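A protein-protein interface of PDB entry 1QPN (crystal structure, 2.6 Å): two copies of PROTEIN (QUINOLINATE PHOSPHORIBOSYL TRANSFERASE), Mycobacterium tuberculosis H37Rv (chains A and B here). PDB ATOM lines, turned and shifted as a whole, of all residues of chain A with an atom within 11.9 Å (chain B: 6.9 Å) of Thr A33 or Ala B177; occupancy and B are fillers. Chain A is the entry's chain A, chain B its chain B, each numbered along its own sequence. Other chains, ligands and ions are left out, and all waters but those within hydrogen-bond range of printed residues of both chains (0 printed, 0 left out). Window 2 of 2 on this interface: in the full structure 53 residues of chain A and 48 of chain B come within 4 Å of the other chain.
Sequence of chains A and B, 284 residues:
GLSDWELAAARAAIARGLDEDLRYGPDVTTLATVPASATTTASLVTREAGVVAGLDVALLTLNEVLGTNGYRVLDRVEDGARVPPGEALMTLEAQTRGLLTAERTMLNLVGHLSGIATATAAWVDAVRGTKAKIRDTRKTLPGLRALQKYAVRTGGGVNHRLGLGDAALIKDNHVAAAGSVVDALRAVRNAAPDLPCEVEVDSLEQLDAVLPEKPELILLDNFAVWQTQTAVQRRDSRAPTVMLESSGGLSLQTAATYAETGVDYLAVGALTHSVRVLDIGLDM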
ATOM      1  N   PRO A  26     -28.607   6.181  16.830  1.00  0.00           N
ATOM      2  CA  PRO A  26     -27.406   6.254  16.000  1.00  0.00           C
ATOM      3  C   PRO A  26     -27.776   6.505  14.565  1.00  0.00           C
ATOM      4  O   PRO A  26     -28.939   6.367  14.165  1.00  0.00           O
ATOM      5  CB  PRO A  26     -26.799   4.870  16.169  1.00  0.00           C
ATOM      6  CG  PRO A  26     -28.022   3.996  16.214  1.00  0.00           C
ATOM      7  CD  PRO A  26     -28.979   4.775  17.097  1.00  0.00           C
ATOM      8  N   ASP A  27     -26.783   6.868  13.777  1.00  0.00           N
ATOM      9  CA  ASP A  27     -27.040   7.126  12.386  1.00  0.00           C
ATOM     10  C   ASP A  27     -27.349   5.781  11.735  1.00  0.00           C
ATOM     11  O   ASP A  27     -26.463   5.122  11.181  1.00  0.00           O
ATOM     12  CB  ASP A  27     -25.812   7.748  11.774  1.00  0.00           C
ATOM     13  CG  ASP A  27     -26.022   8.168  10.345  1.00  0.00           C
ATOM     14  OD1 ASP A  27     -27.181   8.161   9.842  1.00  0.00           O
ATOM     15  OD2 ASP A  27     -24.996   8.525   9.729  1.00  0.00           O
ATOM     16  N   VAL A  28     -28.609   5.381  11.808  1.00  0.00           N
ATOM     17  CA  VAL A  28     -29.064   4.108  11.259  1.00  0.00           C
ATOM     18  C   VAL A  28     -28.715   3.903   9.782  1.00  0.00           C
ATOM     19  O   VAL A  28     -28.410   2.773   9.331  1.00  0.00           O
ATOM     20  CB  VAL A  28     -30.581   3.930  11.539  1.00  0.00           C
ATOM     21  CG1 VAL A  28     -31.265   5.289  11.576  1.00  0.00           C
ATOM     22  CG2 VAL A  28     -31.221   3.042  10.519  1.00  0.00           C
ATOM     23  N   THR A  29     -28.634   5.006   9.054  1.00  0.00           N
ATOM     24  CA  THR A  29     -28.332   4.894   7.644  1.00  0.00           C
ATOM     25  C   THR A  29     -26.873   4.640   7.311  1.00  0.00           C
ATOM     26  O   THR A  29     -26.601   3.947   6.342  1.00  0.00           O
ATOM     27  CB  THR A  29     -28.984   6.026   6.822  1.00  0.00           C
ATOM     28  OG1 THR A  29     -28.387   6.110   5.517  1.00  0.00           O
ATOM     29  CG2 THR A  29     -28.894   7.343   7.561  1.00  0.00           C
ATOM     30  N   THR A  30     -25.924   5.188   8.075  1.00  0.00           N
ATOM     31  CA  THR A  30     -24.514   4.884   7.786  1.00  0.00           C
ATOM     32  C   THR A  30     -24.318   3.445   8.207  1.00  0.00           C
ATOM     33  O   THR A  30     -23.688   2.679   7.502  1.00  0.00           O
ATOM     34  CB  THR A  30     -23.478   5.694   8.584  1.00  0.00           C
ATOM     35  OG1 THR A  30     -23.901   5.852   9.933  1.00  0.00           O
ATOM     36  CG2 THR A  30     -23.251   6.985   7.979  1.00  0.00           C
ATOM     37  N   LEU A  31     -24.850   3.095   9.374  1.00  0.00           N
ATOM     38  CA  LEU A  31     -24.756   1.737   9.897  1.00  0.00           C
ATOM     39  C   LEU A  31     -25.185   0.747   8.835  1.00  0.00           C
ATOM     40  O   LEU A  31     -24.491  -0.232   8.568  1.00  0.00           O
ATOM     41  CB  LEU A  31     -25.668   1.557  11.106  1.00  0.00           C
ATOM     42  CG  LEU A  31     -25.041   1.630  12.485  1.00  0.00           C
ATOM     43  CD1 LEU A  31     -23.962   2.705  12.497  1.00  0.00           C
ATOM     44  CD2 LEU A  31     -26.158   1.946  13.497  1.00  0.00           C
ATOM     45  N   ALA A  32     -26.321   1.023   8.211  1.00  0.00           N
ATOM     46  CA  ALA A  32     -26.838   0.125   7.202  1.00  0.00           C
ATOM     47  C   ALA A  32     -26.034   0.073   5.904  1.00  0.00           C
ATOM     48  O   ALA A  32     -25.877  -0.993   5.326  1.00  0.00           O
ATOM     49  CB  ALA A  32     -28.283   0.454   6.916  1.00  0.00           C
ATOM     50  N   THR A  33     -25.486   1.196   5.465  1.00  0.00           N
ATOM     51  CA  THR A  33     -24.766   1.214   4.200  1.00  0.00           C
ATOM     52  C   THR A  33     -23.237   1.205   4.228  1.00  0.00           C
ATOM     53  O   THR A  33     -22.595   0.844   3.228  1.00  0.00           O
ATOM     54  CB  THR A  33     -25.238   2.404   3.321  1.00  0.00           C
ATOM     55  OG1 THR A  33     -24.863   3.649   3.932  1.00  0.00           O
ATOM     56  CG2 THR A  33     -26.749   2.363   3.173  1.00  0.00           C
ATOM     57  N   VAL A  34     -22.636   1.611   5.341  1.00  0.00           N
ATOM     58  CA  VAL A  34     -21.189   1.658   5.394  1.00  0.00           C
ATOM     59  C   VAL A  34     -20.537   0.754   6.417  1.00  0.00           C
ATOM     60  O   VAL A  34     -20.906   0.727   7.584  1.00  0.00           O
ATOM     61  CB  VAL A  34     -20.611   3.135   5.350  1.00  0.00           C
ATOM     62  CG1 VAL A  34     -21.626   4.124   5.791  1.00  0.00           C
ATOM     63  CG2 VAL A  34     -19.314   3.272   6.126  1.00  0.00           C
ATOM     64  N   PRO A  35     -19.594  -0.072   5.934  1.00  0.00           N
ATOM     65  CA  PRO A  35     -18.852  -1.022   6.749  1.00  0.00           C
ATOM     66  C   PRO A  35     -17.920  -0.376   7.765  1.00  0.00           C
ATOM     67  O   PRO A  35     -17.314   0.675   7.516  1.00  0.00           O
ATOM     68  CB  PRO A  35     -18.115  -1.866   5.697  1.00  0.00           C
ATOM     69  CG  PRO A  35     -17.894  -0.917   4.589  1.00  0.00           C
ATOM     70  CD  PRO A  35     -19.241  -0.245   4.510  1.00  0.00           C
ATOM     71  N   ALA A  36     -17.795  -1.056   8.900  1.00  0.00           N
ATOM     72  CA  ALA A  36     -16.970  -0.588   9.997  1.00  0.00           C
ATOM     73  C   ALA A  36     -15.506  -0.525   9.617  1.00  0.00           C
ATOM     74  O   ALA A  36     -14.759   0.257  10.191  1.00  0.00           O
ATOM     75  CB  ALA A  36     -17.177  -1.463  11.249  1.00  0.00           C
ATOM     76  N   SER A  37     -15.089  -1.309   8.635  1.00  0.00           N
ATOM     77  CA  SER A  37     -13.678  -1.279   8.243  1.00  0.00           C
ATOM     78  C   SER A  37     -13.343  -0.161   7.288  1.00  0.00           C
ATOM     79  O   SER A  37     -12.166   0.084   7.008  1.00  0.00           O
ATOM     80  CB  SER A  37     -13.239  -2.604   7.601  1.00  0.00           C
ATOM     81  OG  SER A  37     -14.217  -3.169   6.737  1.00  0.00           O
ATOM     82  N   ALA A  38     -14.374   0.529   6.803  1.00  0.00           N
ATOM     83  CA  ALA A  38     -14.185   1.586   5.826  1.00  0.00           C
ATOM     84  C   ALA A  38     -13.419   2.789   6.371  1.00  0.00           C
ATOM     85  O   ALA A  38     -13.674   3.266   7.476  1.00  0.00           O
ATOM     86  CB  ALA A  38     -15.529   2.001   5.250  1.00  0.00           C
ATOM     87  N   THR A  39     -12.541   3.314   5.531  1.00  0.00           N
ATOM     88  CA  THR A  39     -11.705   4.432   5.856  1.00  0.00           C
ATOM     89  C   THR A  39     -11.634   5.364   4.652  1.00  0.00           C
ATOM     90  O   THR A  39     -11.516   4.877   3.520  1.00  0.00           O
ATOM     91  CB  THR A  39     -10.359   3.881   6.147  1.00  0.00           C
ATOM     92  OG1 THR A  39     -10.325   3.555   7.528  1.00  0.00           O
ATOM     93  CG2 THR A  39      -9.229   4.821   5.736  1.00  0.00           C
ATOM     94  N   THR A  40     -11.728   6.681   4.891  1.00  0.00           N
ATOM     95  CA  THR A  40     -11.661   7.694   3.828  1.00  0.00           C
ATOM     96  C   THR A  40     -10.729   8.801   4.151  1.00  0.00           C
ATOM     97  O   THR A  40     -10.248   8.940   5.266  1.00  0.00           O
ATOM     98  CB  THR A  40     -12.941   8.472   3.615  1.00  0.00           C
ATOM     99  OG1 THR A  40     -13.787   8.316   4.748  1.00  0.00           O
ATOM    100  CG2 THR A  40     -13.626   8.055   2.377  1.00  0.00           C
ATOM    101  N   GLN A  95     -11.960   6.696   9.841  1.00  0.00           N
ATOM    102  CA  GLN A  95     -12.980   5.701   9.625  1.00  0.00           C
ATOM    103  C   GLN A  95     -14.197   6.442   9.206  1.00  0.00           C
ATOM    104  O   GLN A  95     -14.703   7.246   9.971  1.00  0.00           O
ATOM    105  CB  GLN A  95     -13.282   4.933  10.909  1.00  0.00           C
ATOM    106  CG  GLN A  95     -14.292   3.812  10.725  1.00  0.00           C
ATOM    107  CD  GLN A  95     -15.149   3.608  11.957  1.00  0.00           C
ATOM    108  OE1 GLN A  95     -15.365   4.549  12.743  1.00  0.00           O
ATOM    109  NE2 GLN A  95     -15.680   2.395  12.119  1.00  0.00           N
ATOM    110  N   THR A  96     -14.723   6.070   8.048  1.00  0.00           N
ATOM    111  CA  THR A  96     -15.912   6.671   7.449  1.00  0.00           C
ATOM    112  C   THR A  96     -17.114   6.817   8.375  1.00  0.00           C
ATOM    113  O   THR A  96     -17.737   7.874   8.426  1.00  0.00           O
ATOM    114  CB  THR A  96     -16.321   5.902   6.166  1.00  0.00           C
ATOM    115  OG1 THR A  96     -15.188   5.847   5.290  1.00  0.00           O
ATOM    116  CG2 THR A  96     -17.436   6.624   5.423  1.00  0.00           C
ATOM    117  N   ARG A  97     -17.477   5.772   9.088  1.00  0.00           N
ATOM    118  CA  ARG A  97     -18.620   5.882   9.977  1.00  0.00           C
ATOM    119  C   ARG A  97     -18.422   6.959  11.020  1.00  0.00           C
ATOM    120  O   ARG A  97     -19.363   7.647  11.375  1.00  0.00           O
ATOM    121  CB  ARG A  97     -18.884   4.563  10.701  1.00  0.00           C
ATOM    122  CG  ARG A  97     -19.469   3.446   9.850  1.00  0.00           C
ATOM    123  CD  ARG A  97     -19.703   2.188  10.702  1.00  0.00           C
ATOM    124  NE  ARG A  97     -20.556   1.205  10.048  1.00  0.00           N
ATOM    125  CZ  ARG A  97     -20.978   0.063  10.599  1.00  0.00           C
ATOM    126  NH1 ARG A  97     -20.622  -0.282  11.830  1.00  0.00           N
ATOM    127  NH2 ARG A  97     -21.830  -0.704   9.940  1.00  0.00           N
ATOM    128  N   GLY A  98     -17.205   7.064  11.540  1.00  0.00           N
ATOM    129  CA  GLY A  98     -16.917   8.040  12.573  1.00  0.00           C
ATOM    130  C   GLY A  98     -17.046   9.448  12.057  1.00  0.00           C
ATOM    131  O   GLY A  98     -17.614  10.308  12.746  1.00  0.00           O
ATOM    132  N   LEU A 100     -18.851  10.494   9.533  1.00  0.00           N
ATOM    133  CA  LEU A 100     -20.262  10.811   9.334  1.00  0.00           C
ATOM    134  C   LEU A 100     -21.042  11.130  10.593  1.00  0.00           C
ATOM    135  O   LEU A 100     -22.043  11.838  10.550  1.00  0.00           O
ATOM    136  CB  LEU A 100     -20.942   9.702   8.541  1.00  0.00           C
ATOM    137  CG  LEU A 100     -20.903   9.828   7.008  1.00  0.00           C
ATOM    138  CD1 LEU A 100     -19.766  10.724   6.570  1.00  0.00           C
ATOM    139  CD2 LEU A 100     -20.799   8.446   6.341  1.00  0.00           C
ATOM    140  N   THR A 101     -20.591  10.605  11.715  1.00  0.00           N
ATOM    141  CA  THR A 101     -21.258  10.851  12.994  1.00  0.00           C
ATOM    142  C   THR A 101     -20.841  12.209  13.576  1.00  0.00           C
ATOM    143  O   THR A 101     -21.679  12.955  14.081  1.00  0.00           O
ATOM    144  CB  THR A 101     -20.973   9.672  14.008  1.00  0.00           C
ATOM    145  OG1 THR A 101     -21.735   8.509  13.624  1.00  0.00           O
ATOM    146  CG2 THR A 101     -21.336  10.060  15.441  1.00  0.00           C
ATOM    147  N   GLU A 103     -19.406  14.806  11.775  1.00  0.00           N
ATOM    148  CA  GLU A 103     -19.702  15.826  10.770  1.00  0.00           C
ATOM    149  C   GLU A 103     -20.516  17.057  11.165  1.00  0.00           C
ATOM    150  O   GLU A 103     -19.988  18.165  11.225  1.00  0.00           O
ATOM    151  CB  GLU A 103     -20.367  15.172   9.585  1.00  0.00           C
ATOM    152  CG  GLU A 103     -20.392  16.049   8.395  1.00  0.00           C
ATOM    153  CD  GLU A 103     -21.318  15.537   7.361  1.00  0.00           C
ATOM    154  OE1 GLU A 103     -21.408  14.305   7.207  1.00  0.00           O
ATOM    155  OE2 GLU A 103     -21.988  16.366   6.721  1.00  0.00           O
ATOM    156  N   MET A 284     -15.807  14.206   1.290  1.00  0.00           N
ATOM    157  CA  MET A 284     -15.259  12.845   1.245  1.00  0.00           C
ATOM    158  C   MET A 284     -15.232  12.292  -0.183  1.00  0.00           C
ATOM    159  O   MET A 284     -16.138  12.667  -0.985  1.00  0.00           O
ATOM    160  CB  MET A 284     -16.094  11.915   2.098  1.00  0.00           C
ATOM    161  CG  MET A 284     -15.948  12.219   3.555  1.00  0.00           C
ATOM    162  SD  MET A 284     -17.136  11.314   4.539  1.00  0.00           S
ATOM    163  CE  MET A 284     -17.727  10.167   3.236  1.00  0.00           C
ATOM    164  OXT MET A 284     -14.314  11.471  -0.465  1.00  0.00           O
ATOM    165  N   ILE B 170     -30.623   9.464   3.370  1.00  0.00           N
ATOM    166  CA  ILE B 170     -29.594   8.962   2.468  1.00  0.00           C
ATOM    167  C   ILE B 170     -28.932  10.133   1.768  1.00  0.00           C
ATOM    168  O   ILE B 170     -29.577  10.892   1.053  1.00  0.00           O
ATOM    169  CB  ILE B 170     -30.152   8.001   1.392  1.00  0.00           C
ATOM    170  CG1 ILE B 170     -30.705   6.724   2.031  1.00  0.00           C
ATOM    171  CG2 ILE B 170     -29.045   7.611   0.417  1.00  0.00           C
ATOM    172  CD1 ILE B 170     -32.123   6.826   2.500  1.00  0.00           C
ATOM    173  N   ASP B 172     -25.088  11.579  -0.206  1.00  0.00           N
ATOM    174  CA  ASP B 172     -24.072  11.228  -1.196  1.00  0.00           C
ATOM    175  C   ASP B 172     -23.178  10.071  -0.731  1.00  0.00           C
ATOM    176  O   ASP B 172     -22.997   9.073  -1.437  1.00  0.00           O
ATOM    177  CB  ASP B 172     -23.214  12.470  -1.506  1.00  0.00           C
ATOM    178  CG  ASP B 172     -23.024  13.404  -0.279  1.00  0.00           C
ATOM    179  OD1 ASP B 172     -24.009  14.026   0.196  1.00  0.00           O
ATOM    180  OD2 ASP B 172     -21.874  13.553   0.188  1.00  0.00           O
ATOM    181  N   ASN B 173     -22.678  10.179   0.491  1.00  0.00           N
ATOM    182  CA  ASN B 173     -21.802   9.162   1.051  1.00  0.00           C
ATOM    183  C   ASN B 173     -22.468   7.793   1.063  1.00  0.00           C
ATOM    184  O   ASN B 173     -21.829   6.780   0.806  1.00  0.00           O
ATOM    185  CB  ASN B 173     -21.427   9.502   2.504  1.00  0.00           C
ATOM    186  CG  ASN B 173     -21.318  10.988   2.757  1.00  0.00           C
ATOM    187  OD1 ASN B 173     -20.247  11.589   2.600  1.00  0.00           O
ATOM    188  ND2 ASN B 173     -22.430  11.592   3.165  1.00  0.00           N
ATOM    189  N   HIS B 174     -23.749   7.766   1.398  1.00  0.00           N
ATOM    190  CA  HIS B 174     -24.479   6.509   1.502  1.00  0.00           C
ATOM    191  C   HIS B 174     -24.721   5.857   0.139  1.00  0.00           C
ATOM    192  O   HIS B 174     -24.550   4.644  -0.036  1.00  0.00           O
ATOM    193  CB  HIS B 174     -25.812   6.737   2.239  1.00  0.00           C
ATOM    194  CG  HIS B 174     -25.673   7.527   3.503  1.00  0.00           C
ATOM    195  ND1 HIS B 174     -24.660   7.306   4.411  1.00  0.00           N
ATOM    196  CD2 HIS B 174     -26.399   8.557   3.995  1.00  0.00           C
ATOM    197  CE1 HIS B 174     -24.764   8.172   5.404  1.00  0.00           C
ATOM    198  NE2 HIS B 174     -25.811   8.941   5.174  1.00  0.00           N
ATOM    199  N   VAL B 175     -25.137   6.679  -0.817  1.00  0.00           N
ATOM    200  CA  VAL B 175     -25.420   6.230  -2.173  1.00  0.00           C
ATOM    201  C   VAL B 175     -24.178   5.511  -2.685  1.00  0.00           C
ATOM    202  O   VAL B 175     -24.266   4.418  -3.258  1.00  0.00           O
ATOM    203  CB  VAL B 175     -25.745   7.455  -3.091  1.00  0.00           C
ATOM    204  CG1 VAL B 175     -25.770   7.054  -4.553  1.00  0.00           C
ATOM    205  CG2 VAL B 175     -27.072   8.102  -2.688  1.00  0.00           C
ATOM    206  N   ALA B 176     -23.024   6.129  -2.422  1.00  0.00           N
ATOM    207  CA  ALA B 176     -21.711   5.610  -2.828  1.00  0.00           C
ATOM    208  C   ALA B 176     -21.431   4.219  -2.264  1.00  0.00           C
ATOM    209  O   ALA B 176     -21.123   3.285  -3.000  1.00  0.00           O
ATOM    210  CB  ALA B 176     -20.598   6.582  -2.389  1.00  0.00           C
ATOM    211  N   ALA B 177     -21.524   4.107  -0.945  1.00  0.00           N
ATOM    212  CA  ALA B 177     -21.283   2.860  -0.248  1.00  0.00           C
ATOM    213  C   ALA B 177     -22.238   1.782  -0.702  1.00  0.00           C
ATOM    214  O   ALA B 177     -21.867   0.604  -0.754  1.00  0.00           O
ATOM    215  CB  ALA B 177     -21.419   3.071   1.253  1.00  0.00           C
ATOM    216  N   ALA B 178     -23.478   2.175  -0.979  1.00  0.00           N
ATOM    217  CA  ALA B 178     -24.492   1.224  -1.428  1.00  0.00           C
ATOM    218  C   ALA B 178     -24.266   0.852  -2.891  1.00  0.00           C
ATOM    219  O   ALA B 178     -24.576  -0.265  -3.324  1.00  0.00           O
ATOM    220  CB  ALA B 178     -25.859   1.817  -1.255  1.00  0.00           C
ATOM    221  N   GLY B 179     -23.717   1.801  -3.639  1.00  0.00           N
ATOM    222  CA  GLY B 179     -23.459   1.591  -5.044  1.00  0.00           C
ATOM    223  C   GLY B 179     -24.222   2.665  -5.774  1.00  0.00           C
ATOM    224  O   GLY B 179     -23.667   3.424  -6.575  1.00  0.00           O
ATOM    225  N   SER B 180     -25.498   2.776  -5.432  1.00  0.00           N
ATOM    226  CA  SER B 180     -26.357   3.757  -6.058  1.00  0.00           C
ATOM    227  C   SER B 180     -27.384   4.270  -5.066  1.00  0.00           C
ATOM    228  O   SER B 180     -27.568   3.703  -3.979  1.00  0.00           O
ATOM    229  CB  SER B 180     -27.079   3.145  -7.267  1.00  0.00           C
ATOM    230  OG  SER B 180     -28.036   2.177  -6.857  1.00  0.00           O
ATOM    231  N   ASP B 183     -29.816   1.767  -4.260  1.00  0.00           N
ATOM    232  CA  ASP B 183     -29.174   0.771  -3.429  1.00  0.00           C
ATOM    233  C   ASP B 183     -29.307   1.173  -1.964  1.00  0.00           C
ATOM    234  O   ASP B 183     -29.910   0.442  -1.155  1.00  0.00           O
ATOM    235  CB  ASP B 183     -27.705   0.628  -3.826  1.00  0.00           C
ATOM    236  CG  ASP B 183     -27.514  -0.230  -5.061  1.00  0.00           C
ATOM    237  OD1 ASP B 183     -28.447  -0.991  -5.415  1.00  0.00           O
ATOM    238  OD2 ASP B 183     -26.420  -0.152  -5.672  1.00  0.00           O
ATOM    239  N   ALA B 184     -28.804   2.369  -1.651  1.00  0.00           N
ATOM    240  CA  ALA B 184     -28.847   2.925  -0.297  1.00  0.00           C
ATOM    241  C   ALA B 184     -30.268   2.907   0.221  1.00  0.00           C
ATOM    242  O   ALA B 184     -30.534   2.528   1.357  1.00  0.00           O
ATOM    243  CB  ALA B 184     -28.319   4.347  -0.312  1.00  0.00           C
ATOM    244  N   LEU B 185     -31.186   3.228  -0.667  1.00  0.00           N
ATOM    245  CA  LEU B 185     -32.580   3.293  -0.315  1.00  0.00           C
ATOM    246  C   LEU B 185     -33.128   1.946   0.088  1.00  0.00           C
ATOM    247  O   LEU B 185     -33.742   1.768   1.148  1.00  0.00           O
ATOM    248  CB  LEU B 185     -33.358   3.838  -1.494  1.00  0.00           C
ATOM    249  CG  LEU B 185     -34.319   4.942  -1.125  1.00  0.00           C
ATOM    250  CD1 LEU B 185     -34.889   5.502  -2.387  1.00  0.00           C
ATOM    251  CD2 LEU B 185     -35.387   4.390  -0.230  1.00  0.00           C
ATOM    252  N   ALA B 187     -31.492  -0.751   0.984  1.00  0.00           N
ATOM    253  CA  ALA B 187     -30.782  -1.194   2.178  1.00  0.00           C
ATOM    254  C   ALA B 187     -31.452  -0.655   3.444  1.00  0.00           C
ATOM    255  O   ALA B 187     -31.841  -1.425   4.325  1.00  0.00           O
ATOM    256  CB  ALA B 187     -29.333  -0.720   2.114  1.00  0.00           C
ATOM    257  N   VAL B 188     -31.612   0.667   3.493  1.00  0.00           N
ATOM    258  CA  VAL B 188     -32.228   1.348   4.627  1.00  0.00           C
ATOM    259  C   VAL B 188     -33.682   0.921   4.802  1.00  0.00           C
ATOM    260  O   VAL B 188     -34.161   0.767   5.936  1.00  0.00           O
ATOM    261  CB  VAL B 188     -32.155   2.885   4.479  1.00  0.00           C
ATOM    262  CG1 VAL B 188     -32.795   3.559   5.682  1.00  0.00           C
ATOM    263  CG2 VAL B 188     -30.714   3.314   4.352  1.00  0.00           C
ATOM    264  N   ALA B 191     -33.341  -2.164   6.746  1.00  0.00           N
ATOM    265  CA  ALA B 191     -32.733  -1.992   8.055  1.00  0.00           C
ATOM    266  C   ALA B 191     -33.636  -1.288   9.062  1.00  0.00           C
ATOM    267  O   ALA B 191     -33.665  -1.662  10.227  1.00  0.00           O
ATOM    268  CB  ALA B 191     -31.424  -1.249   7.920  1.00  0.00           C
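The side-chain carboxylate (OD2) of Asp A27 sits at hydrogen-bond distance from the side-chain hydroxyl (OG1) of Thr A30 (2.9 Å). O of Thr A29 sits at hydrogen-bond distance from OG1 of Thr A33 (3.0 Å).
Of chain A, only Thr A33 (3.2 Å) comes within 4 Å of Ala B177. Of chain A, only Thr A29 (3.5 Å), Thr A30 (3.2 Å) and Thr A33 (3.6 Å) come within 4 Å of His B174. No residue of chain A comes within 4 Å of Ala B176. No residue of chain A comes within 4 Å of Ala B178. No residue of chain A comes within 4 Å of Gly B179. No residue of chain A comes within 4 Å of Ala B187. Printed residues of chain A within 4 Å of Asn B173: Met A284 (3.0 Å). Of the printed residues of chain B, Ala A32 touches Ala B191 (3.7 Å). Printed residues of chain A within 4 Å of Val B188: Thr A29. Printed residues of chain B within 4 Å of Met A284: Asn B173 (3.0 Å). Of the printed residues of chain B, Thr A30 touches His B174 (3.2 Å). Ala A36 touches none of the printed residues of chain B. Ser A37 touches none of the printed residues of chain B. The nearest residue of chain B that does not touch Thr A33 is Ala B184 (4.1 Å). The nearest residue of chain A that does not touch Ala B177 is Val A34 (4.2 Å).
Of the 23 printed residues of chain A, 5 touch a printed residue of chain B. Hydrophobic or aromatic side chains of chain A within 4 Å of the printed part of chain B: Ala A32 and Met A284. Of the 16 printed residues of chain B, 5 touch a printed residue of chain A. Hydrophobic or aromatic side chains of chain B that line the printed part of chain A: His B174, Ala B177, Val B188 and Ala B191. Among the printed residues, 7 pairs touch across the chains. Among the printed residues, no Asp or Glu carboxylate lies within 4 Å of a Lys or Arg side-chain nitrogen of the other chain.
No position is printed for both chains. Of the 7 pairs that touch across the chains among the printed residues, none has its exchanged pair printed and touching as well.
Among the printed residues, merely in contact across the chains: Thr A33 with Ala B177, Thr A30 with His B174, Thr A29 with His B174, Thr A33 with His B174, Ala A32 with Ala B191 and Thr A29 with Val B188.
The side-chain sulfur (SD) of Met A284 sits close to the side-chain amide oxygen (OD1) of Asn B173.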
